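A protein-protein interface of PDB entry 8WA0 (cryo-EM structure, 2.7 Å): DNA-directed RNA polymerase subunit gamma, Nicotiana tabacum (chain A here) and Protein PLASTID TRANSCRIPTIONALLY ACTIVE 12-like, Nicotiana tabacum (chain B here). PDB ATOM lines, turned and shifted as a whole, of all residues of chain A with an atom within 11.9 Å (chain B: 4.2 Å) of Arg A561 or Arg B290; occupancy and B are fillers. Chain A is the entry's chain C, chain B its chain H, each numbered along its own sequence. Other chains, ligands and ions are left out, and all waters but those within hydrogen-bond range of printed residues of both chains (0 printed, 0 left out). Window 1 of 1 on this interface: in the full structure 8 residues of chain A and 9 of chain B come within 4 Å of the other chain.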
ATOM      1  N   HIS A 554      32.920  25.164 -22.532  1.00  0.00           N
ATOM      2  CA  HIS A 554      31.938  24.156 -22.142  1.00  0.00           C
ATOM      3  C   HIS A 554      30.566  24.610 -22.609  1.00  0.00           C
ATOM      4  O   HIS A 554      30.221  25.782 -22.466  1.00  0.00           O
ATOM      5  CB  HIS A 554      31.944  24.002 -20.627  1.00  0.00           C
ATOM      6  CG  HIS A 554      33.303  23.749 -20.053  1.00  0.00           C
ATOM      7  ND1 HIS A 554      34.078  24.749 -19.508  1.00  0.00           N
ATOM      8  CD2 HIS A 554      34.026  22.610 -19.941  1.00  0.00           C
ATOM      9  CE1 HIS A 554      35.220  24.237 -19.085  1.00  0.00           C
ATOM     10  NE2 HIS A 554      35.213  22.941 -19.335  1.00  0.00           N
ATOM     11  N   ARG A 555      29.769  23.700 -23.159  1.00  0.00           N
ATOM     12  CA  ARG A 555      28.483  24.118 -23.727  1.00  0.00           C
ATOM     13  C   ARG A 555      27.186  23.930 -22.931  1.00  0.00           C
ATOM     14  O   ARG A 555      26.375  24.852 -22.867  1.00  0.00           O
ATOM     15  CB  ARG A 555      28.334  23.536 -25.136  1.00  0.00           C
ATOM     16  CG  ARG A 555      29.244  24.215 -26.145  1.00  0.00           C
ATOM     17  CD  ARG A 555      29.554  23.323 -27.334  1.00  0.00           C
ATOM     18  NE  ARG A 555      30.560  23.928 -28.202  1.00  0.00           N
ATOM     19  CZ  ARG A 555      31.871  23.752 -28.068  1.00  0.00           C
ATOM     20  NH1 ARG A 555      32.710  24.346 -28.904  1.00  0.00           N
ATOM     21  NH2 ARG A 555      32.346  22.979 -27.100  1.00  0.00           N
ATOM     22  N   GLY A 556      26.964  22.763 -22.334  1.00  0.00           N
ATOM     23  CA  GLY A 556      25.693  22.543 -21.657  1.00  0.00           C
ATOM     24  C   GLY A 556      25.717  22.116 -20.207  1.00  0.00           C
ATOM     25  O   GLY A 556      25.667  22.954 -19.309  1.00  0.00           O
ATOM     26  N   ILE A 557      25.791  20.812 -19.970  1.00  0.00           N
ATOM     27  CA  ILE A 557      25.834  20.295 -18.605  1.00  0.00           C
ATOM     28  C   ILE A 557      27.092  20.776 -17.912  1.00  0.00           C
ATOM     29  O   ILE A 557      27.077  21.048 -16.716  1.00  0.00           O
ATOM     30  CB  ILE A 557      25.710  18.760 -18.549  1.00  0.00           C
ATOM     31  CG1 ILE A 557      26.654  18.095 -19.551  1.00  0.00           C
ATOM     32  CG2 ILE A 557      24.279  18.342 -18.835  1.00  0.00           C
ATOM     33  CD1 ILE A 557      26.589  16.584 -19.530  1.00  0.00           C
ATOM     34  N   CYS A 558      28.184  20.870 -18.658  1.00  0.00           N
ATOM     35  CA  CYS A 558      29.453  21.318 -18.099  1.00  0.00           C
ATOM     36  C   CYS A 558      29.444  22.750 -17.556  1.00  0.00           C
ATOM     37  O   CYS A 558      30.196  23.052 -16.640  1.00  0.00           O
ATOM     38  CB  CYS A 558      30.572  21.135 -19.121  1.00  0.00           C
ATOM     39  SG  CYS A 558      30.794  19.428 -19.672  1.00  0.00           S
ATOM     40  N   VAL A 559      28.666  23.647 -18.158  1.00  0.00           N
ATOM     41  CA  VAL A 559      28.652  25.050 -17.723  1.00  0.00           C
ATOM     42  C   VAL A 559      27.531  25.406 -16.727  1.00  0.00           C
ATOM     43  O   VAL A 559      27.723  26.271 -15.872  1.00  0.00           O
ATOM     44  CB  VAL A 559      28.673  26.006 -18.942  1.00  0.00           C
ATOM     45  CG1 VAL A 559      27.375  25.939 -19.726  1.00  0.00           C
ATOM     46  CG2 VAL A 559      28.995  27.433 -18.527  1.00  0.00           C
ATOM     47  N   ASN A 560      26.375  24.750 -16.808  1.00  0.00           N
ATOM     48  CA  ASN A 560      25.284  25.002 -15.909  1.00  0.00           C
ATOM     49  C   ASN A 560      24.865  23.744 -15.182  1.00  0.00           C
ATOM     50  O   ASN A 560      24.689  22.735 -15.818  1.00  0.00           O
ATOM     51  CB  ASN A 560      24.080  25.529 -16.682  1.00  0.00           C
ATOM     52  CG  ASN A 560      24.380  26.724 -17.532  1.00  0.00           C
ATOM     53  OD1 ASN A 560      24.962  27.699 -17.075  1.00  0.00           O
ATOM     54  ND2 ASN A 560      23.947  26.672 -18.778  1.00  0.00           N
ATOM     55  N   ARG A 561      24.723  23.756 -13.867  1.00  0.00           N
ATOM     56  CA  ARG A 561      24.240  22.611 -13.121  1.00  0.00           C
ATOM     57  C   ARG A 561      22.842  22.196 -13.354  1.00  0.00           C
ATOM     58  O   ARG A 561      22.571  21.018 -13.451  1.00  0.00           O
ATOM     59  CB  ARG A 561      24.405  22.831 -11.637  1.00  0.00           C
ATOM     60  CG  ARG A 561      24.305  21.564 -10.822  1.00  0.00           C
ATOM     61  CD  ARG A 561      24.356  21.804  -9.330  1.00  0.00           C
ATOM     62  NE  ARG A 561      24.084  20.567  -8.613  1.00  0.00           N
ATOM     63  CZ  ARG A 561      24.125  20.435  -7.296  1.00  0.00           C
ATOM     64  NH1 ARG A 561      23.864  19.267  -6.739  1.00  0.00           N
ATOM     65  NH2 ARG A 561      24.432  21.471  -6.535  1.00  0.00           N
ATOM     66  N   TYR A 562      21.930  23.130 -13.463  1.00  0.00           N
ATOM     67  CA  TYR A 562      20.533  22.819 -13.563  1.00  0.00           C
ATOM     68  C   TYR A 562      20.028  23.351 -14.864  1.00  0.00           C
ATOM     69  O   TYR A 562      20.652  24.214 -15.421  1.00  0.00           O
ATOM     70  CB  TYR A 562      19.801  23.427 -12.400  1.00  0.00           C
ATOM     71  CG  TYR A 562      20.111  22.914 -11.034  1.00  0.00           C
ATOM     72  CD1 TYR A 562      19.932  21.590 -10.712  1.00  0.00           C
ATOM     73  CD2 TYR A 562      20.528  23.773 -10.045  1.00  0.00           C
ATOM     74  CE1 TYR A 562      20.202  21.126  -9.447  1.00  0.00           C
ATOM     75  CE2 TYR A 562      20.800  23.320  -8.778  1.00  0.00           C
ATOM     76  CZ  TYR A 562      20.632  21.997  -8.487  1.00  0.00           C
ATOM     77  OH  TYR A 562      20.901  21.544  -7.222  1.00  0.00           O
ATOM     78  N   ASN A 563      18.920  22.859 -15.373  1.00  0.00           N
ATOM     79  CA  ASN A 563      18.450  23.207 -16.698  1.00  0.00           C
ATOM     80  C   ASN A 563      18.246  24.634 -16.774  1.00  0.00           C
ATOM     81  O   ASN A 563      17.688  25.237 -15.875  1.00  0.00           O
ATOM     82  CB  ASN A 563      17.135  22.495 -16.990  1.00  0.00           C
ATOM     83  CG  ASN A 563      16.875  22.248 -18.459  1.00  0.00           C
ATOM     84  OD1 ASN A 563      17.112  23.091 -19.310  1.00  0.00           O
ATOM     85  ND2 ASN A 563      16.332  21.085 -18.753  1.00  0.00           N
ATOM     86  N   PRO A 564      18.673  25.213 -17.854  1.00  0.00           N
ATOM     87  CA  PRO A 564      18.548  26.630 -18.004  1.00  0.00           C
ATOM     88  C   PRO A 564      17.092  27.059 -18.088  1.00  0.00           C
ATOM     89  O   PRO A 564      16.815  28.228 -17.919  1.00  0.00           O
ATOM     90  CB  PRO A 564      19.272  26.855 -19.267  1.00  0.00           C
ATOM     91  CG  PRO A 564      20.387  25.900 -19.233  1.00  0.00           C
ATOM     92  CD  PRO A 564      19.723  24.669 -18.727  1.00  0.00           C
ATOM     93  N   CYS A 565      16.164  26.143 -18.306  1.00  0.00           N
ATOM     94  CA  CYS A 565      14.746  26.447 -18.472  1.00  0.00           C
ATOM     95  C   CYS A 565      14.044  27.114 -17.354  1.00  0.00           C
ATOM     96  O   CYS A 565      13.274  28.040 -17.577  1.00  0.00           O
ATOM     97  CB  CYS A 565      14.009  25.136 -18.661  1.00  0.00           C
ATOM     98  SG  CYS A 565      12.231  25.272 -18.945  1.00  0.00           S
ATOM     99  N   ASN A 566      14.285  26.681 -16.140  1.00  0.00           N
ATOM    100  CA  ASN A 566      13.552  27.231 -15.020  1.00  0.00           C
ATOM    101  C   ASN A 566      13.806  28.718 -14.883  1.00  0.00           C
ATOM    102  O   ASN A 566      12.887  29.482 -14.587  1.00  0.00           O
ATOM    103  CB  ASN A 566      13.903  26.495 -13.729  1.00  0.00           C
ATOM    104  CG  ASN A 566      15.369  26.108 -13.650  1.00  0.00           C
ATOM    105  OD1 ASN A 566      16.259  26.944 -13.811  1.00  0.00           O
ATOM    106  ND2 ASN A 566      15.630  24.834 -13.385  1.00  0.00           N
ATOM    107  N   ARG A 567      15.044  29.137 -15.094  1.00  0.00           N
ATOM    108  CA  ARG A 567      15.370  30.553 -15.023  1.00  0.00           C
ATOM    109  C   ARG A 567      14.845  31.287 -16.252  1.00  0.00           C
ATOM    110  O   ARG A 567      13.955  32.132 -16.149  1.00  0.00           O
ATOM    111  CB  ARG A 567      16.883  30.746 -14.897  1.00  0.00           C
ATOM    112  CG  ARG A 567      17.348  32.195 -14.840  1.00  0.00           C
ATOM    113  CD  ARG A 567      17.091  32.846 -13.485  1.00  0.00           C
ATOM    114  NE  ARG A 567      15.717  33.318 -13.332  1.00  0.00           N
ATOM    115  CZ  ARG A 567      15.302  34.537 -13.663  1.00  0.00           C
ATOM    116  NH1 ARG A 567      14.031  34.874 -13.489  1.00  0.00           N
ATOM    117  NH2 ARG A 567      16.155  35.420 -14.164  1.00  0.00           N
ATOM    118  N   LYS A 585      26.868  34.527 -24.033  1.00  0.00           N
ATOM    119  CA  LYS A 585      26.800  34.997 -22.670  1.00  0.00           C
ATOM    120  C   LYS A 585      26.597  36.486 -22.649  1.00  0.00           C
ATOM    121  O   LYS A 585      26.411  37.096 -23.680  1.00  0.00           O
ATOM    122  CB  LYS A 585      28.052  34.602 -21.901  1.00  0.00           C
ATOM    123  CG  LYS A 585      27.851  34.411 -20.403  1.00  0.00           C
ATOM    124  CD  LYS A 585      29.109  33.898 -19.723  1.00  0.00           C
ATOM    125  CE  LYS A 585      29.099  32.381 -19.633  1.00  0.00           C
ATOM    126  NZ  LYS A 585      30.312  31.854 -18.949  1.00  0.00           N
ATOM    127  N   GLN B 271      25.664  18.298  -0.705  1.00  0.00           N
ATOM    128  CA  GLN B 271      25.675  18.870  -2.032  1.00  0.00           C
ATOM    129  C   GLN B 271      25.261  17.890  -3.119  1.00  0.00           C
ATOM    130  O   GLN B 271      24.739  18.309  -4.135  1.00  0.00           O
ATOM    131  CB  GLN B 271      27.045  19.465  -2.308  1.00  0.00           C
ATOM    132  CG  GLN B 271      27.107  20.539  -3.376  1.00  0.00           C
ATOM    133  CD  GLN B 271      28.459  21.222  -3.406  1.00  0.00           C
ATOM    134  OE1 GLN B 271      28.713  22.096  -4.228  1.00  0.00           O
ATOM    135  NE2 GLN B 271      29.334  20.824  -2.498  1.00  0.00           N
ATOM    136  N   LEU B 286      31.034  10.877 -14.066  1.00  0.00           N
ATOM    137  CA  LEU B 286      30.292  12.098 -14.145  1.00  0.00           C
ATOM    138  C   LEU B 286      30.959  13.235 -13.391  1.00  0.00           C
ATOM    139  O   LEU B 286      30.894  14.367 -13.827  1.00  0.00           O
ATOM    140  CB  LEU B 286      28.851  11.851 -13.722  1.00  0.00           C
ATOM    141  CG  LEU B 286      27.760  12.849 -13.995  1.00  0.00           C
ATOM    142  CD1 LEU B 286      27.429  12.808 -15.467  1.00  0.00           C
ATOM    143  CD2 LEU B 286      26.569  12.430 -13.173  1.00  0.00           C
ATOM    144  N   TYR B 287      31.569  12.974 -12.260  1.00  0.00           N
ATOM    145  CA  TYR B 287      32.284  13.974 -11.524  1.00  0.00           C
ATOM    146  C   TYR B 287      33.422  14.563 -12.279  1.00  0.00           C
ATOM    147  O   TYR B 287      33.657  15.754 -12.180  1.00  0.00           O
ATOM    148  CB  TYR B 287      32.741  13.474 -10.181  1.00  0.00           C
ATOM    149  CG  TYR B 287      33.434  14.456  -9.288  1.00  0.00           C
ATOM    150  CD1 TYR B 287      32.718  15.339  -8.522  1.00  0.00           C
ATOM    151  CD2 TYR B 287      34.807  14.467  -9.178  1.00  0.00           C
ATOM    152  CE1 TYR B 287      33.349  16.233  -7.700  1.00  0.00           C
ATOM    153  CE2 TYR B 287      35.444  15.356  -8.359  1.00  0.00           C
ATOM    154  CZ  TYR B 287      34.708  16.233  -7.626  1.00  0.00           C
ATOM    155  OH  TYR B 287      35.341  17.124  -6.806  1.00  0.00           O
ATOM    156  N   ARG B 288      34.139  13.784 -13.037  1.00  0.00           N
ATOM    157  CA  ARG B 288      35.253  14.285 -13.746  1.00  0.00           C
ATOM    158  C   ARG B 288      34.738  15.333 -14.711  1.00  0.00           C
ATOM    159  O   ARG B 288      35.384  16.351 -14.893  1.00  0.00           O
ATOM    160  CB  ARG B 288      35.964  13.134 -14.393  1.00  0.00           C
ATOM    161  CG  ARG B 288      37.450  13.272 -14.572  1.00  0.00           C
ATOM    162  CD  ARG B 288      37.937  12.091 -15.376  1.00  0.00           C
ATOM    163  NE  ARG B 288      37.656  10.836 -14.705  1.00  0.00           N
ATOM    164  CZ  ARG B 288      37.352   9.711 -15.334  1.00  0.00           C
ATOM    165  NH1 ARG B 288      37.265   9.692 -16.649  1.00  0.00           N
ATOM    166  NH2 ARG B 288      37.121   8.607 -14.645  1.00  0.00           N
ATOM    167  N   ALA B 289      33.611  15.117 -15.339  1.00  0.00           N
ATOM    168  CA  ALA B 289      32.961  16.075 -16.199  1.00  0.00           C
ATOM    169  C   ALA B 289      32.406  17.325 -15.578  1.00  0.00           C
ATOM    170  O   ALA B 289      32.484  18.370 -16.174  1.00  0.00           O
ATOM    171  CB  ALA B 289      31.874  15.358 -16.888  1.00  0.00           C
ATOM    172  N   ARG B 290      31.827  17.252 -14.421  1.00  0.00           N
ATOM    173  CA  ARG B 290      31.213  18.366 -13.778  1.00  0.00           C
ATOM    174  C   ARG B 290      31.896  18.904 -12.537  1.00  0.00           C
ATOM    175  O   ARG B 290      31.263  19.570 -11.770  1.00  0.00           O
ATOM    176  CB  ARG B 290      29.801  17.963 -13.435  1.00  0.00           C
ATOM    177  CG  ARG B 290      28.990  17.380 -14.562  1.00  0.00           C
ATOM    178  CD  ARG B 290      27.582  17.146 -14.083  1.00  0.00           C
ATOM    179  NE  ARG B 290      26.661  18.111 -14.643  1.00  0.00           N
ATOM    180  CZ  ARG B 290      25.654  18.656 -13.986  1.00  0.00           C
ATOM    181  NH1 ARG B 290      24.869  19.519 -14.593  1.00  0.00           N
ATOM    182  NH2 ARG B 290      25.439  18.347 -12.727  1.00  0.00           N
ATOM    183  N   ARG B 291      33.162  18.645 -12.324  1.00  0.00           N
ATOM    184  CA  ARG B 291      33.916  19.052 -11.158  1.00  0.00           C
ATOM    185  C   ARG B 291      34.003  20.532 -10.908  1.00  0.00           C
ATOM    186  O   ARG B 291      34.021  20.954  -9.778  1.00  0.00           O
ATOM    187  CB  ARG B 291      35.314  18.527 -11.417  1.00  0.00           C
ATOM    188  CG  ARG B 291      36.239  18.391 -10.240  1.00  0.00           C
ATOM    189  CD  ARG B 291      37.499  17.752 -10.779  1.00  0.00           C
ATOM    190  NE  ARG B 291      37.453  17.772 -12.233  1.00  0.00           N
ATOM    191  CZ  ARG B 291      38.437  17.365 -13.020  1.00  0.00           C
ATOM    192  NH1 ARG B 291      39.554  16.901 -12.489  1.00  0.00           N
ATOM    193  NH2 ARG B 291      38.310  17.422 -14.332  1.00  0.00           N
ATOM    194  N   HIS B 292      34.116  21.325 -11.935  1.00  0.00           N
ATOM    195  CA  HIS B 292      34.213  22.749 -11.849  1.00  0.00           C
ATOM    196  C   HIS B 292      33.000  23.434 -11.310  1.00  0.00           C
ATOM    197  O   HIS B 292      33.117  24.397 -10.579  1.00  0.00           O
ATOM    198  CB  HIS B 292      34.483  23.219 -13.246  1.00  0.00           C
ATOM    199  CG  HIS B 292      35.552  22.451 -13.946  1.00  0.00           C
ATOM    200  ND1 HIS B 292      35.279  21.551 -14.952  1.00  0.00           N
ATOM    201  CD2 HIS B 292      36.895  22.445 -13.788  1.00  0.00           C
ATOM    202  CE1 HIS B 292      36.409  21.022 -15.384  1.00  0.00           C
ATOM    203  NE2 HIS B 292      37.405  21.549 -14.695  1.00  0.00           N
ATOM    204  N   LEU B 293      31.825  22.957 -11.646  1.00  0.00           N
ATOM    205  CA  LEU B 293      30.605  23.576 -11.250  1.00  0.00           C
ATOM    206  C   LEU B 293      30.497  23.598  -9.773  1.00  0.00           C
ATOM    207  O   LEU B 293      30.133  24.591  -9.201  1.00  0.00           O
ATOM    208  CB  LEU B 293      29.485  22.816 -11.898  1.00  0.00           C
ATOM    209  CG  LEU B 293      29.463  22.776 -13.398  1.00  0.00           C
ATOM    210  CD1 LEU B 293      28.251  21.997 -13.837  1.00  0.00           C
ATOM    211  CD2 LEU B 293      29.384  24.210 -13.860  1.00  0.00           C
ATOM    212  N   TYR B 294      30.862  22.540  -9.126  1.00  0.00           N
ATOM    213  CA  TYR B 294      30.906  22.466  -7.698  1.00  0.00           C
ATOM    214  C   TYR B 294      31.935  23.300  -6.933  1.00  0.00           C
ATOM    215  O   TYR B 294      31.597  23.810  -5.883  1.00  0.00           O
ATOM    216  CB  TYR B 294      30.916  21.018  -7.299  1.00  0.00           C
ATOM    217  CG  TYR B 294      29.890  20.175  -7.976  1.00  0.00           C
ATOM    218  CD1 TYR B 294      28.551  20.312  -7.689  1.00  0.00           C
ATOM    219  CD2 TYR B 294      30.266  19.216  -8.887  1.00  0.00           C
ATOM    220  CE1 TYR B 294      27.614  19.525  -8.312  1.00  0.00           C
ATOM    221  CE2 TYR B 294      29.338  18.428  -9.513  1.00  0.00           C
ATOM    222  CZ  TYR B 294      28.022  18.595  -9.221  1.00  0.00           C
ATOM    223  OH  TYR B 294      27.108  17.810  -9.846  1.00  0.00           O
ATOM    224  N   GLU B 297      30.598  26.821  -6.778  1.00  0.00           N
ATOM    225  CA  GLU B 297      29.595  26.982  -5.782  1.00  0.00           C
ATOM    226  C   GLU B 297      30.156  27.103  -4.399  1.00  0.00           C
ATOM    227  O   GLU B 297      29.700  27.922  -3.625  1.00  0.00           O
ATOM    228  CB  GLU B 297      28.626  25.850  -5.869  1.00  0.00           C
ATOM    229  CG  GLU B 297      27.754  25.850  -7.101  1.00  0.00           C
ATOM    230  CD  GLU B 297      26.780  24.695  -7.102  1.00  0.00           C
ATOM    231  OE1 GLU B 297      26.729  23.965  -6.094  1.00  0.00           O
ATOM    232  OE2 GLU B 297      26.065  24.519  -8.109  1.00  0.00           O
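The backbone carbonyl oxygen (O) of Ile A557 is in hydrogen-bond range of the guanidinium group (NH1) of Arg B290 (3.4 Å).
O of Asn A560 lies within hydrogen-bond range of NH1 of Arg B290 (3.4 Å).
O of Gln B271 lies within hydrogen-bond range of NH1 of Arg A561, 2.9 Å away.
The backbone carbonyl oxygen (O) of Arg A561 sits at hydrogen-bond distance from the guanidinium group (NH1) of Arg B290 (3.0 Å).
The guanidinium group (NH2) of Arg A561 is in salt-bridge range of the side-chain carboxylate (OE1) of Glu B297 (3.4 Å).
The side-chain carboxylate (OE1) of Glu B297 lies close to the side-chain amide oxygen (OE1) of Gln B271 (3.3 Å).
NH2 of Arg B290 is in hydrogen-bond range of OH of Tyr B294 (3.4 Å).
Ile A557 touches Leu B293 (O to CD1, 3.3 Å).
O of Cys A558 touches CD2 of Leu B293, at 3.1 Å.
Val A559 touches Leu B293 (O to CD2, 3.3 Å).
Leu B293 touches Arg A561.
Arg A561 touches Tyr B294.
Of the 11 printed residues of chain B, 5 touch a printed residue of chain A.
Of the 15 printed residues of chain A, 5 touch a printed residue of chain B.
Among the printed residues, 10 pairs touch across the chains.
Among the printed residues, Asp or Glu carboxylates within 4 Å of a Lys or Arg side-chain nitrogen of the other chain: Arg A561 with Glu B297.
Gln B271 touches just one residue of chain A: Arg A561 (2.9 Å).
No residue of chain A comes within 4 Å of Tyr B287.
No residue of chain A comes within 4 Å of His B292.
Of the printed residues of chain A, Glu B297 touches Arg A561.
Printed residues of chain B within 4 Å of Ile A557: Arg B290 and Leu B293.
Of the printed residues of chain B, Cys A558 touches Leu B293 (3.1 Å).
Of the printed residues of chain B, Asn A560 touches Arg B290.
The nearest printed residue of chain B that does not touch Arg A561 is His B292 (8.6 Å).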
